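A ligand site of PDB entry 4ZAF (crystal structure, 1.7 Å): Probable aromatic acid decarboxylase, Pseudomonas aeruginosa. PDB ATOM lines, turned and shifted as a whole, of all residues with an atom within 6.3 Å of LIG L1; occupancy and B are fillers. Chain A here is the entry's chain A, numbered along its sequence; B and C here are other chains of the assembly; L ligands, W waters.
Water W1 lies within hydrogen-bond range of O3 of LIG L1, O of Ala 141 of chain B, NH1 of Arg 139 of chain B and NH1 of Arg 185 of chain C.
N of Gly 91 is in hydrogen-bond range of O1 of LIG L1 (2.8 Å).
The guanidinium group of Arg 122 is in salt-bridge range of an oxygen (O2) of LIG L1, at 3.0 Å.
The guanidinium group (NH2) of Arg 185 of chain C lies within salt-bridge range of an oxygen (O1) of LIG L1 (2.6 Å).
OG of Ser 90 lies within hydrogen-bond range of O4 of LIG L1.
The side-chain carboxylate (OE1) of Glu 140 of chain B lies close to an oxygen (O2) of LIG L1, 2.4 Å away.
O of Arg 139 of chain B sits at hydrogen-bond distance from N2 of LG2 L2.
OH of Tyr 169 of chain C sits at hydrogen-bond distance from O3 of LIG L1 (2.8 Å).
O2 of LG2 L2 sits at hydrogen-bond distance from NH2 of Arg 139 of chain B, 2.7 Å away.
NZ of Lys 129 is in salt-bridge range of O1 of LIG L1 (2.7 Å).
An oxygen (O2) of LG2 L2 lies within hydrogen-bond range of the backbone NH (N) of Ser 15 of chain B.
An oxygen (O1) of LG2 L2 lies within hydrogen-bond range of the guanidinium group of Arg 122 (3.5 Å).
The guanidinium group (NH2) of Arg 139 of chain B lies within salt-bridge range of an oxygen (O3) of LIG L1, 3.0 Å away.
NZ of Lys 129 lies within salt-bridge range of OE2 of Glu 130, 2.8 Å away.
NE of Arg 122 is in hydrogen-bond range of O of Ala 89, at 2.9 Å.
NZ of Lys 129 sits at hydrogen-bond distance from O of Ala 141 of chain B.
The guanidinium group of Arg 185 of chain C lies within hydrogen-bond range of the backbone carbonyl oxygen of Ala 141 of chain B, 3.3 Å away.
The indole nitrogen of Trp 200 of chain C lies close to the backbone carbonyl oxygen of Ala 86, at 3.5 Å.
N of Tyr 169 of chain C sits at hydrogen-bond distance from OG of Ser 15 of chain B (3.4 Å).
NH2 of Arg 185 of chain C is in salt-bridge range of OE2 of Glu 130 (3.1 Å).
The side-chain carboxylate (OE2) of Glu 140 of chain B lies within salt-bridge range of the guanidinium group (NH1) of Arg 122 (2.9 Å).
O of Trp 84 touches C5 of LIG L1 (3.4 Å).
O of Ala 89 touches C2 of LIG L1, 3.6 Å away.
Ser 92 touches LIG L1.
Trp 200 of chain C touches LIG L1 (CE2 to C4, 3.7 Å).
Hydrophobic or aromatic side chains that line LIG L1: Ala 89, Tyr 169 of chain C and Trp 200 of chain C.
12 residues have an atom within 4 Å of LIG L1: Trp 84, Ala 89, Ser 90, Gly 91, Ser 92, Arg 122, Lys 129, Arg 139 of chain B, Glu 140 of chain B, Tyr 169 of chain C, Arg 185 of chain C and Trp 200 of chain C.
The nearest printed residue that does not touch LIG L1 is Glu 130 (4.2 Å).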
ATOM      1  N   TRP A  84      24.566 -13.077  -5.536  1.00  0.00           N
ATOM      2  CA  TRP A  84      24.933 -13.015  -4.134  1.00  0.00           C
ATOM      3  C   TRP A  84      25.654 -14.271  -3.621  1.00  0.00           C
ATOM      4  O   TRP A  84      26.236 -14.261  -2.572  1.00  0.00           O
ATOM      5  CB  TRP A  84      23.705 -12.691  -3.256  1.00  0.00           C
ATOM      6  CG  TRP A  84      22.861 -11.565  -3.788  1.00  0.00           C
ATOM      7  CD1 TRP A  84      21.585 -11.647  -4.236  1.00  0.00           C
ATOM      8  CD2 TRP A  84      23.258 -10.213  -3.985  1.00  0.00           C
ATOM      9  NE1 TRP A  84      21.181 -10.444  -4.747  1.00  0.00           N
ATOM     10  CE2 TRP A  84      22.189  -9.536  -4.581  1.00  0.00           C
ATOM     11  CE3 TRP A  84      24.461  -9.493  -3.744  1.00  0.00           C
ATOM     12  CZ2 TRP A  84      22.244  -8.199  -4.909  1.00  0.00           C
ATOM     13  CZ3 TRP A  84      24.487  -8.137  -4.056  1.00  0.00           C
ATOM     14  CH2 TRP A  84      23.440  -7.547  -4.697  1.00  0.00           C
ATOM     15  N   MET A  85      25.663 -15.343  -4.399  1.00  0.00           N
ATOM     16  CA  MET A  85      26.446 -16.537  -4.035  1.00  0.00           C
ATOM     17  C   MET A  85      27.927 -16.437  -4.373  1.00  0.00           C
ATOM     18  O   MET A  85      28.704 -17.289  -4.032  1.00  0.00           O
ATOM     19  CB  MET A  85      25.798 -17.779  -4.769  1.00  0.00           C
ATOM     20  CG  MET A  85      24.314 -17.970  -4.474  1.00  0.00           C
ATOM     21  SD  MET A  85      23.658 -17.621  -2.771  1.00  0.00           S
ATOM     22  CE  MET A  85      22.105 -16.785  -3.123  1.00  0.00           C
ATOM     23  N   ALA A  86      28.355 -15.356  -5.048  1.00  0.00           N
ATOM     24  CA  ALA A  86      29.740 -15.084  -5.367  1.00  0.00           C
ATOM     25  C   ALA A  86      30.525 -14.574  -4.175  1.00  0.00           C
ATOM     26  O   ALA A  86      29.959 -13.900  -3.322  1.00  0.00           O
ATOM     27  CB  ALA A  86      29.795 -14.109  -6.477  1.00  0.00           C
ATOM     28  N   ALA A  89      30.325 -10.943  -2.360  1.00  0.00           N
ATOM     29  CA  ALA A  89      29.089 -10.500  -1.702  1.00  0.00           C
ATOM     30  C   ALA A  89      29.154 -10.622  -0.158  1.00  0.00           C
ATOM     31  O   ALA A  89      28.297 -10.034   0.530  1.00  0.00           O
ATOM     32  CB  ALA A  89      27.922 -11.287  -2.215  1.00  0.00           C
ATOM     33  N   SER A  90      30.101 -11.406   0.379  1.00  0.00           N
ATOM     34  CA  SER A  90      30.235 -11.690   1.809  1.00  0.00           C
ATOM     35  C   SER A  90      31.602 -11.435   2.351  1.00  0.00           C
ATOM     36  O   SER A  90      32.612 -11.762   1.749  1.00  0.00           O
ATOM     37  CB  SER A  90      29.887 -13.121   2.154  1.00  0.00           C
ATOM     38  OG  SER A  90      30.020 -13.407   3.516  1.00  0.00           O
ATOM     39  N   GLY A  91      31.627 -10.837   3.555  1.00  0.00           N
ATOM     40  CA  GLY A  91      32.887 -10.682   4.214  1.00  0.00           C
ATOM     41  C   GLY A  91      33.464 -11.983   4.754  1.00  0.00           C
ATOM     42  O   GLY A  91      34.560 -11.984   5.200  1.00  0.00           O
ATOM     43  N   SER A  92      32.688 -13.074   4.747  1.00  0.00           N
ATOM     44  CA  SER A  92      33.253 -14.357   5.139  1.00  0.00           C
ATOM     45  C   SER A  92      34.000 -15.012   3.999  1.00  0.00           C
ATOM     46  O   SER A  92      34.521 -16.112   4.193  1.00  0.00           O
ATOM     47  CB  SER A  92      32.110 -15.295   5.614  1.00  0.00           C
ATOM     48  OG  SER A  92      31.285 -15.680   4.539  1.00  0.00           O
ATOM     49  N   ARG A 122      27.788  -3.947  -3.458  1.00  0.00           N
ATOM     50  CA  ARG A 122      27.887  -4.769  -2.275  1.00  0.00           C
ATOM     51  C   ARG A 122      29.300  -5.186  -2.041  1.00  0.00           C
ATOM     52  O   ARG A 122      29.761  -5.253  -0.888  1.00  0.00           O
ATOM     53  CB  ARG A 122      26.972  -6.002  -2.384  1.00  0.00           C
ATOM     54  CG  ARG A 122      27.087  -7.012  -1.242  1.00  0.00           C
ATOM     55  CD  ARG A 122      26.777  -6.490   0.137  1.00  0.00           C
ATOM     56  NE  ARG A 122      26.963  -7.550   1.099  1.00  0.00           N
ATOM     57  CZ  ARG A 122      26.856  -7.395   2.393  1.00  0.00           C
ATOM     58  NH1 ARG A 122      26.560  -6.184   2.930  1.00  0.00           N
ATOM     59  NH2 ARG A 122      27.128  -8.468   3.158  1.00  0.00           N
ATOM     60  N   VAL A 126      31.466  -4.525   1.323  1.00  0.00           N
ATOM     61  CA  VAL A 126      32.133  -5.598   2.088  1.00  0.00           C
ATOM     62  C   VAL A 126      33.634  -5.267   2.249  1.00  0.00           C
ATOM     63  O   VAL A 126      34.213  -5.440   3.317  1.00  0.00           O
ATOM     64  CB  VAL A 126      31.972  -6.919   1.327  1.00  0.00           C
ATOM     65  CG1 VAL A 126      32.918  -7.982   1.876  1.00  0.00           C
ATOM     66  CG2 VAL A 126      30.540  -7.380   1.463  1.00  0.00           C
ATOM     67  N   LYS A 129      33.890  -2.740   5.128  1.00  0.00           N
ATOM     68  CA  LYS A 129      33.625  -3.274   6.447  1.00  0.00           C
ATOM     69  C   LYS A 129      34.657  -4.266   6.981  1.00  0.00           C
ATOM     70  O   LYS A 129      34.871  -4.326   8.200  1.00  0.00           O
ATOM     71  CB  LYS A 129      32.194  -3.846   6.547  1.00  0.00           C
ATOM     72  CG  LYS A 129      32.050  -5.304   6.027  1.00  0.00           C
ATOM     73  CD  LYS A 129      30.585  -5.677   5.917  1.00  0.00           C
ATOM     74  CE  LYS A 129      30.397  -7.109   5.426  1.00  0.00           C
ATOM     75  NZ  LYS A 129      30.730  -8.051   6.535  1.00  0.00           N
ATOM     76  N   GLU A 130      35.290  -4.952   6.036  1.00  0.00           N
ATOM     77  CA  GLU A 130      36.365  -5.903   6.339  1.00  0.00           C
ATOM     78  C   GLU A 130      37.769  -5.305   6.344  1.00  0.00           C
ATOM     79  O   GLU A 130      38.738  -6.003   6.638  1.00  0.00           O
ATOM     80  CB  GLU A 130      36.286  -7.074   5.413  1.00  0.00           C
ATOM     81  CG  GLU A 130      35.032  -7.872   5.478  1.00  0.00           C
ATOM     82  CD  GLU A 130      34.608  -8.515   6.789  1.00  0.00           C
ATOM     83  OE1 GLU A 130      35.458  -8.846   7.628  1.00  0.00           O
ATOM     84  OE2 GLU A 130      33.408  -8.726   6.937  1.00  0.00           O
ATOM     85  N   SER B  15      20.731 -11.569   6.262  1.00  0.00           N
ATOM     86  CA  SER B  15      20.595 -12.856   6.925  1.00  0.00           C
ATOM     87  C   SER B  15      19.748 -12.624   8.141  1.00  0.00           C
ATOM     88  O   SER B  15      19.734 -11.541   8.800  1.00  0.00           O
ATOM     89  CB  SER B  15      21.970 -13.428   7.233  1.00  0.00           C
ATOM     90  OG  SER B  15      21.848 -14.739   7.727  1.00  0.00           O
ATOM     91  N   ARG B 139      21.334  -6.610  10.348  1.00  0.00           N
ATOM     92  CA  ARG B 139      22.144  -7.826  10.629  1.00  0.00           C
ATOM     93  C   ARG B 139      23.401  -7.776   9.780  1.00  0.00           C
ATOM     94  O   ARG B 139      23.314  -7.953   8.574  1.00  0.00           O
ATOM     95  CB  ARG B 139      21.336  -9.117  10.336  1.00  0.00           C
ATOM     96  CG  ARG B 139      21.785 -10.416  11.066  1.00  0.00           C
ATOM     97  CD  ARG B 139      23.280 -10.698  11.174  1.00  0.00           C
ATOM     98  NE  ARG B 139      23.887 -10.838   9.923  1.00  0.00           N
ATOM     99  CZ  ARG B 139      25.199 -10.968   9.653  1.00  0.00           C
ATOM    100  NH1 ARG B 139      26.177 -11.090  10.547  1.00  0.00           N
ATOM    101  NH2 ARG B 139      25.520 -10.938   8.392  1.00  0.00           N
ATOM    102  N   GLU B 140      24.505  -7.423  10.402  1.00  0.00           N
ATOM    103  CA  GLU B 140      25.750  -7.243   9.681  1.00  0.00           C
ATOM    104  C   GLU B 140      26.848  -7.283  10.720  1.00  0.00           C
ATOM    105  O   GLU B 140      26.642  -6.945  11.859  1.00  0.00           O
ATOM    106  CB  GLU B 140      25.738  -5.926   8.873  1.00  0.00           C
ATOM    107  CG  GLU B 140      27.014  -5.716   8.010  1.00  0.00           C
ATOM    108  CD  GLU B 140      27.245  -6.803   7.031  1.00  0.00           C
ATOM    109  OE1 GLU B 140      27.857  -7.844   7.443  1.00  0.00           O
ATOM    110  OE2 GLU B 140      26.916  -6.664   5.815  1.00  0.00           O
ATOM    111  N   ALA B 141      28.040  -7.752  10.322  1.00  0.00           N
ATOM    112  CA  ALA B 141      29.217  -7.633  11.136  1.00  0.00           C
ATOM    113  C   ALA B 141      30.450  -7.857  10.299  1.00  0.00           C
ATOM    114  O   ALA B 141      30.410  -8.729   9.406  1.00  0.00           O
ATOM    115  CB  ALA B 141      29.164  -8.636  12.323  1.00  0.00           C
ATOM    116  N   PRO B 142      31.496  -7.061  10.469  1.00  0.00           N
ATOM    117  CA  PRO B 142      31.507  -5.790  11.221  1.00  0.00           C
ATOM    118  C   PRO B 142      30.579  -4.789  10.641  1.00  0.00           C
ATOM    119  O   PRO B 142      30.169  -4.973   9.494  1.00  0.00           O
ATOM    120  CB  PRO B 142      32.932  -5.247  11.013  1.00  0.00           C
ATOM    121  CG  PRO B 142      33.701  -6.419  10.556  1.00  0.00           C
ATOM    122  CD  PRO B 142      32.816  -7.417   9.938  1.00  0.00           C
ATOM    123  N   GLY C 167      24.958 -14.443  11.755  1.00  0.00           N
ATOM    124  CA  GLY C 167      24.260 -14.781  10.531  1.00  0.00           C
ATOM    125  C   GLY C 167      23.707 -16.172  10.600  1.00  0.00           C
ATOM    126  O   GLY C 167      24.197 -17.001  11.384  1.00  0.00           O
ATOM    127  N   TYR C 169      23.206 -17.870   7.482  1.00  0.00           N
ATOM    128  CA  TYR C 169      23.279 -18.389   6.153  1.00  0.00           C
ATOM    129  C   TYR C 169      24.078 -19.699   6.068  1.00  0.00           C
ATOM    130  O   TYR C 169      24.210 -20.249   4.991  1.00  0.00           O
ATOM    131  CB  TYR C 169      23.859 -17.329   5.213  1.00  0.00           C
ATOM    132  CG  TYR C 169      25.146 -16.616   5.643  1.00  0.00           C
ATOM    133  CD1 TYR C 169      26.385 -17.190   5.480  1.00  0.00           C
ATOM    134  CD2 TYR C 169      25.112 -15.347   6.216  1.00  0.00           C
ATOM    135  CE1 TYR C 169      27.545 -16.514   5.771  1.00  0.00           C
ATOM    136  CE2 TYR C 169      26.272 -14.687   6.591  1.00  0.00           C
ATOM    137  CZ  TYR C 169      27.488 -15.243   6.321  1.00  0.00           C
ATOM    138  OH  TYR C 169      28.612 -14.502   6.634  1.00  0.00           O
ATOM    139  N   PHE C 181      29.685 -18.578  14.919  1.00  0.00           N
ATOM    140  CA  PHE C 181      29.644 -17.624  13.793  1.00  0.00           C
ATOM    141  C   PHE C 181      30.406 -16.314  14.184  1.00  0.00           C
ATOM    142  O   PHE C 181      31.271 -15.837  13.453  1.00  0.00           O
ATOM    143  CB  PHE C 181      28.189 -17.316  13.365  1.00  0.00           C
ATOM    144  CG  PHE C 181      28.099 -16.416  12.164  1.00  0.00           C
ATOM    145  CD1 PHE C 181      28.319 -15.067  12.296  1.00  0.00           C
ATOM    146  CD2 PHE C 181      27.761 -16.899  10.898  1.00  0.00           C
ATOM    147  CE1 PHE C 181      28.299 -14.237  11.205  1.00  0.00           C
ATOM    148  CE2 PHE C 181      27.719 -16.065   9.806  1.00  0.00           C
ATOM    149  CZ  PHE C 181      27.983 -14.728   9.984  1.00  0.00           C
ATOM    150  N   ARG C 185      34.099 -14.725  12.860  1.00  0.00           N
ATOM    151  CA  ARG C 185      34.300 -13.437  12.227  1.00  0.00           C
ATOM    152  C   ARG C 185      35.357 -12.640  12.937  1.00  0.00           C
ATOM    153  O   ARG C 185      36.113 -11.923  12.291  1.00  0.00           O
ATOM    154  CB  ARG C 185      32.980 -12.663  12.181  1.00  0.00           C
ATOM    155  CG  ARG C 185      31.923 -13.343  11.369  1.00  0.00           C
ATOM    156  CD  ARG C 185      32.368 -13.628   9.972  1.00  0.00           C
ATOM    157  NE  ARG C 185      32.378 -12.433   9.153  1.00  0.00           N
ATOM    158  CZ  ARG C 185      31.527 -12.222   8.166  1.00  0.00           C
ATOM    159  NH1 ARG C 185      30.595 -13.100   7.924  1.00  0.00           N
ATOM    160  NH2 ARG C 185      31.598 -11.135   7.463  1.00  0.00           N
ATOM    161  N   TRP C 200      32.814 -18.018   1.981  1.00  0.00           N
ATOM    162  CA  TRP C 200      31.703 -17.893   1.105  1.00  0.00           C
ATOM    163  C   TRP C 200      32.046 -17.890  -0.388  1.00  0.00           C
ATOM    164  O   TRP C 200      32.903 -17.149  -0.824  1.00  0.00           O
ATOM    165  CB  TRP C 200      30.938 -16.570   1.417  1.00  0.00           C
ATOM    166  CG  TRP C 200      29.689 -16.366   0.682  1.00  0.00           C
ATOM    167  CD1 TRP C 200      29.499 -15.597  -0.447  1.00  0.00           C
ATOM    168  CD2 TRP C 200      28.427 -16.961   0.935  1.00  0.00           C
ATOM    169  NE1 TRP C 200      28.225 -15.650  -0.846  1.00  0.00           N
ATOM    170  CE2 TRP C 200      27.534 -16.519  -0.036  1.00  0.00           C
ATOM    171  CE3 TRP C 200      27.951 -17.850   1.918  1.00  0.00           C
ATOM    172  CZ2 TRP C 200      26.211 -16.890  -0.069  1.00  0.00           C
ATOM    173  CZ3 TRP C 200      26.634 -18.236   1.869  1.00  0.00           C
ATOM    174  CH2 TRP C 200      25.771 -17.782   0.886  1.00  0.00           C
HETATM  175  O1  LIG L   1      29.847 -10.450   5.618  1.00  0.00           O
HETATM  176  P1  LIG L   1      28.431 -10.919   5.787  1.00  0.00           P
HETATM  177  O2  LIG L   1      27.484  -9.671   5.855  1.00  0.00           O
HETATM  178  O3  LIG L   1      28.096 -11.751   6.978  1.00  0.00           O
HETATM  179  O4  LIG L   1      27.969 -11.640   4.429  1.00  0.00           O
HETATM  180  C1  LIG L   1      26.561 -11.884   4.354  1.00  0.00           C
HETATM  181  C2  LIG L   1      26.260 -11.867   2.845  1.00  0.00           C
HETATM  182  C3  LIG L   1      26.200 -13.150   2.074  1.00  0.00           C
HETATM  183  C4  LIG L   1      26.334 -14.497   2.765  1.00  0.00           C
HETATM  184  C5  LIG L   1      25.977 -13.036   0.573  1.00  0.00           C
HETATM  185  N1  LG2 L   2      23.351  -8.118   3.211  1.00  0.00           N
HETATM  186  C1  LG2 L   2      23.474  -7.570   4.497  1.00  0.00           C
HETATM  187  O1  LG2 L   2      23.524  -6.300   4.608  1.00  0.00           O
HETATM  188  N2  LG2 L   2      23.565  -8.331   5.601  1.00  0.00           N
HETATM  189  C2  LG2 L   2      23.518  -9.723   5.516  1.00  0.00           C
HETATM  190  O2  LG2 L   2      23.551 -10.420   6.553  1.00  0.00           O
HETATM  191  C3  LG2 L   2      23.331 -10.286   4.240  1.00  0.00           C
HETATM  192  N3  LG2 L   2      23.247 -11.678   4.160  1.00  0.00           N
HETATM  193  C4  LG2 L   2      22.917 -12.147   2.927  1.00  0.00           C
HETATM  194  C5  LG2 L   2      22.710 -13.535   2.825  1.00  0.00           C
HETATM  195  C6  LG2 L   2      22.390 -14.101   1.589  1.00  0.00           C
HETATM  196  C7  LG2 L   2      22.208 -15.554   1.506  1.00  0.00           C
HETATM  197  C8  LG2 L   2      22.244 -13.316   0.488  1.00  0.00           C
HETATM  198  C9  LG2 L   2      21.935 -13.893  -0.796  1.00  0.00           C
HETATM  199  C10 LG2 L   2      22.503 -11.907   0.539  1.00  0.00           C
HETATM  200  C11 LG2 L   2      22.836 -11.324   1.775  1.00  0.00           C
HETATM  201  N4  LG2 L   2      23.098  -9.995   1.909  1.00  0.00           N
HETATM  202  C12 LG2 L   2      23.256  -9.495   3.089  1.00  0.00           C
HETATM  203  C13 LG2 L   2      23.125  -9.126   0.691  1.00  0.00           C
HETATM  204  C14 LG2 L   2      21.975  -8.402   0.135  1.00  0.00           C
HETATM  205  O3  LG2 L   2      20.916  -9.289   0.077  1.00  0.00           O
HETATM  206  C15 LG2 L   2      22.319  -7.433  -0.921  1.00  0.00           C
HETATM  207  O4  LG2 L   2      23.271  -6.386  -0.582  1.00  0.00           O
HETATM  208  C16 LG2 L   2      21.039  -6.848  -1.439  1.00  0.00           C
HETATM  209  O5  LG2 L   2      21.390  -5.868  -2.483  1.00  0.00           O
HETATM  210  C17 LG2 L   2      20.103  -6.275  -0.419  1.00  0.00           C
HETATM  211  O6  LG2 L   2      18.976  -5.791  -1.179  1.00  0.00           O
HETATM  212  P1  LG2 L   2      17.609  -5.395  -0.431  1.00  0.00           P
HETATM  213  O7  LG2 L   2      16.729  -4.786  -1.558  1.00  0.00           O
HETATM  214  O8  LG2 L   2      16.968  -6.602   0.250  1.00  0.00           O
HETATM  215  O9  LG2 L   2      17.997  -4.295   0.623  1.00  0.00           O
HETATM  216  O   HOH W   1      28.895 -11.080   9.426  1.00  0.00           O
